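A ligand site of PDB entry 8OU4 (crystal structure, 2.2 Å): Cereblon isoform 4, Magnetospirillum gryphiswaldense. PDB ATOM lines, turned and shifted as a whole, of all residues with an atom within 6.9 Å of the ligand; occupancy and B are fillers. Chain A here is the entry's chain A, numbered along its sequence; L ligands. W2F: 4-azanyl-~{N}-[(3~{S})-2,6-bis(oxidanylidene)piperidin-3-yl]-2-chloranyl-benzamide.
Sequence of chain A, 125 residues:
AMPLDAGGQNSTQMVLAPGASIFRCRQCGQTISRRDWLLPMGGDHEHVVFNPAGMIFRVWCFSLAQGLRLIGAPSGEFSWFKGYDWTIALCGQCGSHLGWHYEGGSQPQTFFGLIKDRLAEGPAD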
ATOM      1  N   VAL A  49      -3.619  -4.046   5.979  1.00  0.00           N
ATOM      2  CA  VAL A  49      -3.448  -5.431   5.559  1.00  0.00           C
ATOM      3  C   VAL A  49      -1.978  -5.690   5.270  1.00  0.00           C
ATOM      4  O   VAL A  49      -1.219  -4.739   5.066  1.00  0.00           O
ATOM      5  CB  VAL A  49      -4.322  -5.740   4.322  1.00  0.00           C
ATOM      6  CG1 VAL A  49      -5.808  -5.661   4.632  1.00  0.00           C
ATOM      7  CG2 VAL A  49      -3.985  -4.828   3.143  1.00  0.00           C
ATOM      8  N   PHE A  50      -1.587  -6.971   5.247  1.00  0.00           N
ATOM      9  CA  PHE A  50      -0.252  -7.355   4.779  1.00  0.00           C
ATOM     10  C   PHE A  50      -0.360  -8.502   3.782  1.00  0.00           C
ATOM     11  O   PHE A  50      -1.234  -9.357   3.902  1.00  0.00           O
ATOM     12  CB  PHE A  50       0.678  -7.691   5.947  1.00  0.00           C
ATOM     13  CG  PHE A  50       0.364  -8.938   6.731  1.00  0.00           C
ATOM     14  CD1 PHE A  50      -0.548  -8.910   7.774  1.00  0.00           C
ATOM     15  CD2 PHE A  50       1.024 -10.126   6.458  1.00  0.00           C
ATOM     16  CE1 PHE A  50      -0.809 -10.051   8.509  1.00  0.00           C
ATOM     17  CE2 PHE A  50       0.763 -11.267   7.194  1.00  0.00           C
ATOM     18  CZ  PHE A  50      -0.155 -11.229   8.224  1.00  0.00           C
ATOM     19  N   ASN A  51       0.547  -8.498   2.789  1.00  0.00           N
ATOM     20  CA  ASN A  51       0.573  -9.492   1.728  1.00  0.00           C
ATOM     21  C   ASN A  51       1.560 -10.600   2.123  1.00  0.00           C
ATOM     22  O   ASN A  51       2.223 -10.493   3.146  1.00  0.00           O
ATOM     23  CB  ASN A  51       0.870  -8.821   0.384  1.00  0.00           C
ATOM     24  CG  ASN A  51       2.301  -8.345   0.220  1.00  0.00           C
ATOM     25  OD1 ASN A  51       3.180  -8.682   1.012  1.00  0.00           O
ATOM     26  ND2 ASN A  51       2.575  -7.599  -0.827  1.00  0.00           N
ATOM     27  N   PRO A  52       1.652 -11.715   1.352  1.00  0.00           N
ATOM     28  CA  PRO A  52       2.576 -12.820   1.683  1.00  0.00           C
ATOM     29  C   PRO A  52       4.058 -12.445   1.666  1.00  0.00           C
ATOM     30  O   PRO A  52       4.882 -13.193   2.187  1.00  0.00           O
ATOM     31  CB  PRO A  52       2.311 -13.879   0.600  1.00  0.00           C
ATOM     32  CG  PRO A  52       0.945 -13.515   0.034  1.00  0.00           C
ATOM     33  CD  PRO A  52       0.860 -12.007   0.153  1.00  0.00           C
ATOM     34  N   ALA A  53       4.388 -11.307   1.038  1.00  0.00           N
ATOM     35  CA  ALA A  53       5.753 -10.806   1.010  1.00  0.00           C
ATOM     36  C   ALA A  53       6.013  -9.886   2.212  1.00  0.00           C
ATOM     37  O   ALA A  53       7.085  -9.288   2.314  1.00  0.00           O
ATOM     38  CB  ALA A  53       6.005 -10.082  -0.287  1.00  0.00           C
ATOM     39  N   GLY A  54       5.013  -9.745   3.095  1.00  0.00           N
ATOM     40  CA  GLY A  54       5.193  -9.080   4.373  1.00  0.00           C
ATOM     41  C   GLY A  54       5.043  -7.561   4.280  1.00  0.00           C
ATOM     42  O   GLY A  54       5.309  -6.853   5.247  1.00  0.00           O
ATOM     43  N   MET A  55       4.604  -7.080   3.116  1.00  0.00           N
ATOM     44  CA  MET A  55       4.399  -5.660   2.891  1.00  0.00           C
ATOM     45  C   MET A  55       3.077  -5.265   3.542  1.00  0.00           C
ATOM     46  O   MET A  55       2.066  -5.927   3.315  1.00  0.00           O
ATOM     47  CB  MET A  55       4.340  -5.343   1.394  1.00  0.00           C
ATOM     48  CG  MET A  55       5.661  -5.508   0.683  1.00  0.00           C
ATOM     49  SD  MET A  55       5.547  -5.110  -1.077  1.00  0.00           S
ATOM     50  CE  MET A  55       7.060  -5.855  -1.686  1.00  0.00           C
ATOM     51  N   PHE A  57       0.088  -2.495   3.893  1.00  0.00           N
ATOM     52  CA  PHE A  57      -0.573  -1.438   3.155  1.00  0.00           C
ATOM     53  C   PHE A  57      -1.757  -0.928   3.976  1.00  0.00           C
ATOM     54  O   PHE A  57      -2.484  -1.716   4.577  1.00  0.00           O
ATOM     55  CB  PHE A  57      -1.102  -1.936   1.808  1.00  0.00           C
ATOM     56  CG  PHE A  57      -0.091  -2.558   0.889  1.00  0.00           C
ATOM     57  CD1 PHE A  57       0.762  -1.778   0.131  1.00  0.00           C
ATOM     58  CD2 PHE A  57       0.006  -3.936   0.780  1.00  0.00           C
ATOM     59  CE1 PHE A  57       1.680  -2.355  -0.726  1.00  0.00           C
ATOM     60  CE2 PHE A  57       0.934  -4.513  -0.073  1.00  0.00           C
ATOM     61  CZ  PHE A  57       1.766  -3.723  -0.828  1.00  0.00           C
ATOM     62  N   SER A  75      -7.644 -13.077  -9.558  1.00  0.00           N
ATOM     63  CA  SER A  75      -7.136 -14.166  -8.744  1.00  0.00           C
ATOM     64  C   SER A  75      -7.743 -14.080  -7.347  1.00  0.00           C
ATOM     65  O   SER A  75      -7.899 -12.995  -6.796  1.00  0.00           O
ATOM     66  CB  SER A  75      -5.631 -14.142  -8.691  1.00  0.00           C
ATOM     67  OG  SER A  75      -5.129 -15.150  -7.818  1.00  0.00           O
ATOM     68  N   GLU A  77      -6.409 -15.893  -4.767  1.00  0.00           N
ATOM     69  CA  GLU A  77      -5.360 -16.298  -3.832  1.00  0.00           C
ATOM     70  C   GLU A  77      -4.997 -15.115  -2.929  1.00  0.00           C
ATOM     71  O   GLU A  77      -4.665 -14.046  -3.417  1.00  0.00           O
ATOM     72  CB  GLU A  77      -4.131 -16.789  -4.596  1.00  0.00           C
ATOM     73  N   PHE A  78      -5.093 -15.336  -1.615  1.00  0.00           N
ATOM     74  CA  PHE A  78      -4.651 -14.397  -0.605  1.00  0.00           C
ATOM     75  C   PHE A  78      -5.491 -13.113  -0.628  1.00  0.00           C
ATOM     76  O   PHE A  78      -4.992 -12.053  -0.268  1.00  0.00           O
ATOM     77  CB  PHE A  78      -3.163 -14.054  -0.767  1.00  0.00           C
ATOM     78  CG  PHE A  78      -2.213 -15.223  -0.646  1.00  0.00           C
ATOM     79  CD1 PHE A  78      -2.238 -16.041   0.466  1.00  0.00           C
ATOM     80  CD2 PHE A  78      -1.259 -15.463  -1.627  1.00  0.00           C
ATOM     81  CE1 PHE A  78      -1.356 -17.106   0.582  1.00  0.00           C
ATOM     82  CE2 PHE A  78      -0.370 -16.528  -1.498  1.00  0.00           C
ATOM     83  CZ  PHE A  78      -0.423 -17.345  -0.395  1.00  0.00           C
ATOM     84  N   SER A  79      -6.764 -13.212  -1.034  1.00  0.00           N
ATOM     85  CA  SER A  79      -7.639 -12.056  -1.065  1.00  0.00           C
ATOM     86  C   SER A  79      -7.975 -11.633   0.361  1.00  0.00           C
ATOM     87  O   SER A  79      -8.406 -12.444   1.178  1.00  0.00           O
ATOM     88  CB  SER A  79      -8.897 -12.331  -1.852  1.00  0.00           C
ATOM     89  OG  SER A  79      -9.727 -11.177  -1.889  1.00  0.00           O
ATOM     90  N   TRP A  80      -7.780 -10.338   0.655  1.00  0.00           N
ATOM     91  CA  TRP A  80      -8.067  -9.769   1.957  1.00  0.00           C
ATOM     92  C   TRP A  80      -9.577  -9.670   2.184  1.00  0.00           C
ATOM     93  O   TRP A  80     -10.029  -9.554   3.316  1.00  0.00           O
ATOM     94  CB  TRP A  80      -7.406  -8.400   2.100  1.00  0.00           C
ATOM     95  CG  TRP A  80      -5.916  -8.436   2.065  1.00  0.00           C
ATOM     96  CD1 TRP A  80      -5.085  -9.211   2.842  1.00  0.00           C
ATOM     97  CD2 TRP A  80      -5.058  -7.638   1.234  1.00  0.00           C
ATOM     98  NE1 TRP A  80      -3.775  -8.951   2.537  1.00  0.00           N
ATOM     99  CE2 TRP A  80      -3.725  -7.993   1.556  1.00  0.00           C
ATOM    100  CE3 TRP A  80      -5.282  -6.665   0.255  1.00  0.00           C
ATOM    101  CZ2 TRP A  80      -2.641  -7.394   0.934  1.00  0.00           C
ATOM    102  CZ3 TRP A  80      -4.199  -6.086  -0.367  1.00  0.00           C
ATOM    103  CH2 TRP A  80      -2.892  -6.450  -0.032  1.00  0.00           C
ATOM    104  N   PHE A  81     -10.349  -9.702   1.090  1.00  0.00           N
ATOM    105  CA  PHE A  81     -11.788  -9.538   1.149  1.00  0.00           C
ATOM    106  C   PHE A  81     -12.454 -10.840   0.687  1.00  0.00           C
ATOM    107  O   PHE A  81     -12.351 -11.218  -0.482  1.00  0.00           O
ATOM    108  CB  PHE A  81     -12.204  -8.334   0.300  1.00  0.00           C
ATOM    109  CG  PHE A  81     -11.567  -7.040   0.753  1.00  0.00           C
ATOM    110  CD1 PHE A  81     -12.053  -6.352   1.848  1.00  0.00           C
ATOM    111  CD2 PHE A  81     -10.461  -6.532   0.088  1.00  0.00           C
ATOM    112  CE1 PHE A  81     -11.487  -5.155   2.248  1.00  0.00           C
ATOM    113  CE2 PHE A  81      -9.880  -5.336   0.504  1.00  0.00           C
ATOM    114  CZ  PHE A  81     -10.391  -4.648   1.580  1.00  0.00           C
ATOM    115  N   TYR A  84     -14.135 -12.194  -2.904  1.00  0.00           N
ATOM    116  CA  TYR A  84     -13.682 -11.348  -4.000  1.00  0.00           C
ATOM    117  C   TYR A  84     -12.359 -11.852  -4.574  1.00  0.00           C
ATOM    118  O   TYR A  84     -11.482 -12.290  -3.823  1.00  0.00           O
ATOM    119  CB  TYR A  84     -13.511  -9.900  -3.550  1.00  0.00           C
ATOM    120  CG  TYR A  84     -14.786  -9.220  -3.154  1.00  0.00           C
ATOM    121  CD1 TYR A  84     -15.619  -8.626  -4.106  1.00  0.00           C
ATOM    122  CD2 TYR A  84     -15.169  -9.156  -1.828  1.00  0.00           C
ATOM    123  CE1 TYR A  84     -16.792  -7.992  -3.738  1.00  0.00           C
ATOM    124  CE2 TYR A  84     -16.338  -8.521  -1.438  1.00  0.00           C
ATOM    125  CZ  TYR A  84     -17.160  -7.959  -2.396  1.00  0.00           C
ATOM    126  OH  TYR A  84     -18.308  -7.335  -2.008  1.00  0.00           O
ATOM    127  N   TRP A  86      -9.080 -10.555  -7.115  1.00  0.00           N
ATOM    128  CA  TRP A  86      -8.406  -9.279  -7.271  1.00  0.00           C
ATOM    129  C   TRP A  86      -7.623  -9.233  -8.581  1.00  0.00           C
ATOM    130  O   TRP A  86      -7.163 -10.253  -9.084  1.00  0.00           O
ATOM    131  CB  TRP A  86      -7.501  -8.982  -6.066  1.00  0.00           C
ATOM    132  CG  TRP A  86      -6.503 -10.061  -5.763  1.00  0.00           C
ATOM    133  CD1 TRP A  86      -6.613 -11.017  -4.792  1.00  0.00           C
ATOM    134  CD2 TRP A  86      -5.231 -10.273  -6.395  1.00  0.00           C
ATOM    135  NE1 TRP A  86      -5.508 -11.824  -4.798  1.00  0.00           N
ATOM    136  CE2 TRP A  86      -4.649 -11.398  -5.776  1.00  0.00           C
ATOM    137  CE3 TRP A  86      -4.533  -9.639  -7.433  1.00  0.00           C
ATOM    138  CZ2 TRP A  86      -3.403 -11.896  -6.155  1.00  0.00           C
ATOM    139  CZ3 TRP A  86      -3.299 -10.137  -7.805  1.00  0.00           C
ATOM    140  CH2 TRP A  86      -2.741 -11.250  -7.174  1.00  0.00           C
ATOM    141  N   THR A  87      -7.507  -8.013  -9.125  1.00  0.00           N
ATOM    142  CA  THR A  87      -6.619  -7.710 -10.238  1.00  0.00           C
ATOM    143  C   THR A  87      -5.786  -6.496  -9.843  1.00  0.00           C
ATOM    144  O   THR A  87      -6.281  -5.583  -9.191  1.00  0.00           O
ATOM    145  CB  THR A  87      -7.408  -7.453 -11.525  1.00  0.00           C
ATOM    146  OG1 THR A  87      -8.296  -6.353 -11.306  1.00  0.00           O
ATOM    147  CG2 THR A  87      -8.205  -8.658 -11.993  1.00  0.00           C
ATOM    148  N   ILE A  88      -4.515  -6.506 -10.259  1.00  0.00           N
ATOM    149  CA  ILE A  88      -3.606  -5.417  -9.951  1.00  0.00           C
ATOM    150  C   ILE A  88      -4.090  -4.169 -10.687  1.00  0.00           C
ATOM    151  O   ILE A  88      -4.446  -4.243 -11.861  1.00  0.00           O
ATOM    152  CB  ILE A  88      -2.157  -5.786 -10.349  1.00  0.00           C
ATOM    153  CG1 ILE A  88      -1.664  -7.045  -9.641  1.00  0.00           C
ATOM    154  CG2 ILE A  88      -1.231  -4.609 -10.080  1.00  0.00           C
ATOM    155  CD1 ILE A  88      -0.489  -7.713 -10.303  1.00  0.00           C
ATOM    156  N   HIS A  97       1.904   1.289  -9.145  1.00  0.00           N
ATOM    157  CA  HIS A  97       0.952   0.373  -8.554  1.00  0.00           C
ATOM    158  C   HIS A  97       0.130   1.107  -7.490  1.00  0.00           C
ATOM    159  O   HIS A  97       0.681   1.510  -6.470  1.00  0.00           O
ATOM    160  CB  HIS A  97       1.668  -0.859  -7.972  1.00  0.00           C
ATOM    161  CG  HIS A  97       0.753  -1.786  -7.241  1.00  0.00           C
ATOM    162  ND1 HIS A  97       1.105  -2.433  -6.091  1.00  0.00           N
ATOM    163  CD2 HIS A  97      -0.488  -2.196  -7.532  1.00  0.00           C
ATOM    164  CE1 HIS A  97       0.098  -3.198  -5.691  1.00  0.00           C
ATOM    165  NE2 HIS A  97      -0.882  -3.067  -6.554  1.00  0.00           N
ATOM    166  N   TRP A 100      -5.693  -2.496  -6.123  1.00  0.00           N
ATOM    167  CA  TRP A 100      -6.319  -3.642  -6.746  1.00  0.00           C
ATOM    168  C   TRP A 100      -7.791  -3.350  -7.039  1.00  0.00           C
ATOM    169  O   TRP A 100      -8.425  -2.559  -6.335  1.00  0.00           O
ATOM    170  CB  TRP A 100      -6.185  -4.902  -5.884  1.00  0.00           C
ATOM    171  CG  TRP A 100      -4.789  -5.189  -5.426  1.00  0.00           C
ATOM    172  CD1 TRP A 100      -3.921  -6.100  -5.963  1.00  0.00           C
ATOM    173  CD2 TRP A 100      -4.089  -4.582  -4.320  1.00  0.00           C
ATOM    174  NE1 TRP A 100      -2.737  -6.093  -5.279  1.00  0.00           N
ATOM    175  CE2 TRP A 100      -2.815  -5.177  -4.264  1.00  0.00           C
ATOM    176  CE3 TRP A 100      -4.426  -3.603  -3.374  1.00  0.00           C
ATOM    177  CZ2 TRP A 100      -1.863  -4.805  -3.310  1.00  0.00           C
ATOM    178  CZ3 TRP A 100      -3.477  -3.231  -2.441  1.00  0.00           C
ATOM    179  CH2 TRP A 100      -2.216  -3.826  -2.411  1.00  0.00           C
ATOM    180  N   TYR A 102     -11.416  -5.328  -7.130  1.00  0.00           N
ATOM    181  CA  TYR A 102     -12.031  -6.523  -6.575  1.00  0.00           C
ATOM    182  C   TYR A 102     -13.321  -6.805  -7.330  1.00  0.00           C
ATOM    183  O   TYR A 102     -14.051  -5.880  -7.665  1.00  0.00           O
ATOM    184  CB  TYR A 102     -12.237  -6.336  -5.066  1.00  0.00           C
ATOM    185  CG  TYR A 102     -10.951  -6.384  -4.283  1.00  0.00           C
ATOM    186  CD1 TYR A 102     -10.400  -7.589  -3.895  1.00  0.00           C
ATOM    187  CD2 TYR A 102     -10.263  -5.224  -3.967  1.00  0.00           C
ATOM    188  CE1 TYR A 102      -9.215  -7.642  -3.187  1.00  0.00           C
ATOM    189  CE2 TYR A 102      -9.083  -5.256  -3.241  1.00  0.00           C
ATOM    190  CZ  TYR A 102      -8.549  -6.471  -2.869  1.00  0.00           C
ATOM    191  OH  TYR A 102      -7.361  -6.535  -2.171  1.00  0.00           O
HETATM  192  N1  W2F L   1      -4.143  -9.712  -1.134  1.00  0.00           N
HETATM  193  N2  W2F L   1      -0.991  -9.963  -2.956  1.00  0.00           N
HETATM  194  C3  W2F L   1      -5.007  -9.026  -1.951  1.00  0.00           C
HETATM  195  C4  W2F L   1      -4.429  -8.428  -3.198  1.00  0.00           C
HETATM  196  C5  W2F L   1      -3.168  -9.138  -3.682  1.00  0.00           C
HETATM  197  C7  W2F L   1       1.391 -10.299  -3.358  1.00  0.00           C
HETATM  198  C9  W2F L   1       2.344 -12.447  -3.979  1.00  0.00           C
HETATM  199  C11 W2F L   1       3.786 -10.583  -3.513  1.00  0.00           C
HETATM  200  C12 W2F L   1       2.693  -9.784  -3.260  1.00  0.00           C
HETATM  201  C1  W2F L   1      -2.175  -9.237  -2.542  1.00  0.00           C
HETATM  202  C2  W2F L   1      -2.783  -9.874  -1.304  1.00  0.00           C
HETATM  203  C6  W2F L   1       0.226  -9.395  -3.069  1.00  0.00           C
HETATM  204  O1  W2F L   1       0.398  -8.191  -2.907  1.00  0.00           O
HETATM  205  C8  W2F L   1       1.238 -11.637  -3.720  1.00  0.00           C
HETATM  206  C10 W2F L   1       3.625 -11.921  -3.879  1.00  0.00           C
HETATM  207  N3  W2F L   1       4.728 -12.721  -4.128  1.00  0.00           N
HETATM  208 CL1  W2F L   1      -0.330 -12.359  -3.870  1.00  0.00          CL
HETATM  209  O2  W2F L   1      -6.178  -8.923  -1.663  1.00  0.00           O
HETATM  210  O3  W2F L   1      -2.124 -10.490  -0.495  1.00  0.00           O
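CD of Pro 52 touches O3 of the ligand (3.4 Å).
CB of Ala 53 touches C11 of the ligand, 3.9 Å away.
Ser 79 touches the ligand.
Trp 86 touches the ligand (CE2 to C5, 3.4 Å).
NE1 of Trp 100 touches C5 of the ligand, at 3.5 Å.
Hydrophobic or aromatic side chains within 4 Å of the ligand: Pro 52, Ala 53, Phe 78, Trp 80, Trp 86, Trp 100 and Tyr 102.
Within 4 Å of the ligand: Asn 51, Pro 52, Ala 53, Phe 78, Ser 79, Trp 80, Trp 86, Trp 100 and Tyr 102.
O of Phe 78 is in hydrogen-bond range of N1 of the ligand.
OH of Tyr 102 lies within hydrogen-bond range of O2 of the ligand, at 2.7 Å.
The side-chain amide nitrogen of Asn 51 lies within hydrogen-bond range of an oxygen (O1) of the ligand (3.1 Å).
O2 of the ligand sits close to N of Trp 80 (3.2 Å).
The side-chain amide oxygen (OD1) of Asn 51 lies within hydrogen-bond range of the backbone NH (N) of Ala 53 (2.9 Å).
The side-chain amide oxygen (OD1) of Asn 51 is in hydrogen-bond range of the backbone NH (N) of Met 55.
The side-chain amide oxygen (OD1) of Asn 51 lies within hydrogen-bond range of the backbone NH (N) of Gly 54 (3.0 Å).
The indole nitrogen (NE1) of Trp 80 is in hydrogen-bond range of the backbone carbonyl oxygen (O) of Phe 50, at 2.9 Å.
The indole nitrogen of Trp 86 sits at hydrogen-bond distance from the backbone carbonyl oxygen of Glu 77.
The backbone carbonyl oxygen of Ser 75 sits at hydrogen-bond distance from the backbone NH of Trp 86, 2.7 Å away.
O of Phe 81 lies within hydrogen-bond range of OG of Ser 79 (3.0 Å).
OG of Ser 79 lies within hydrogen-bond range of O of Tyr 84, at 2.8 Å.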
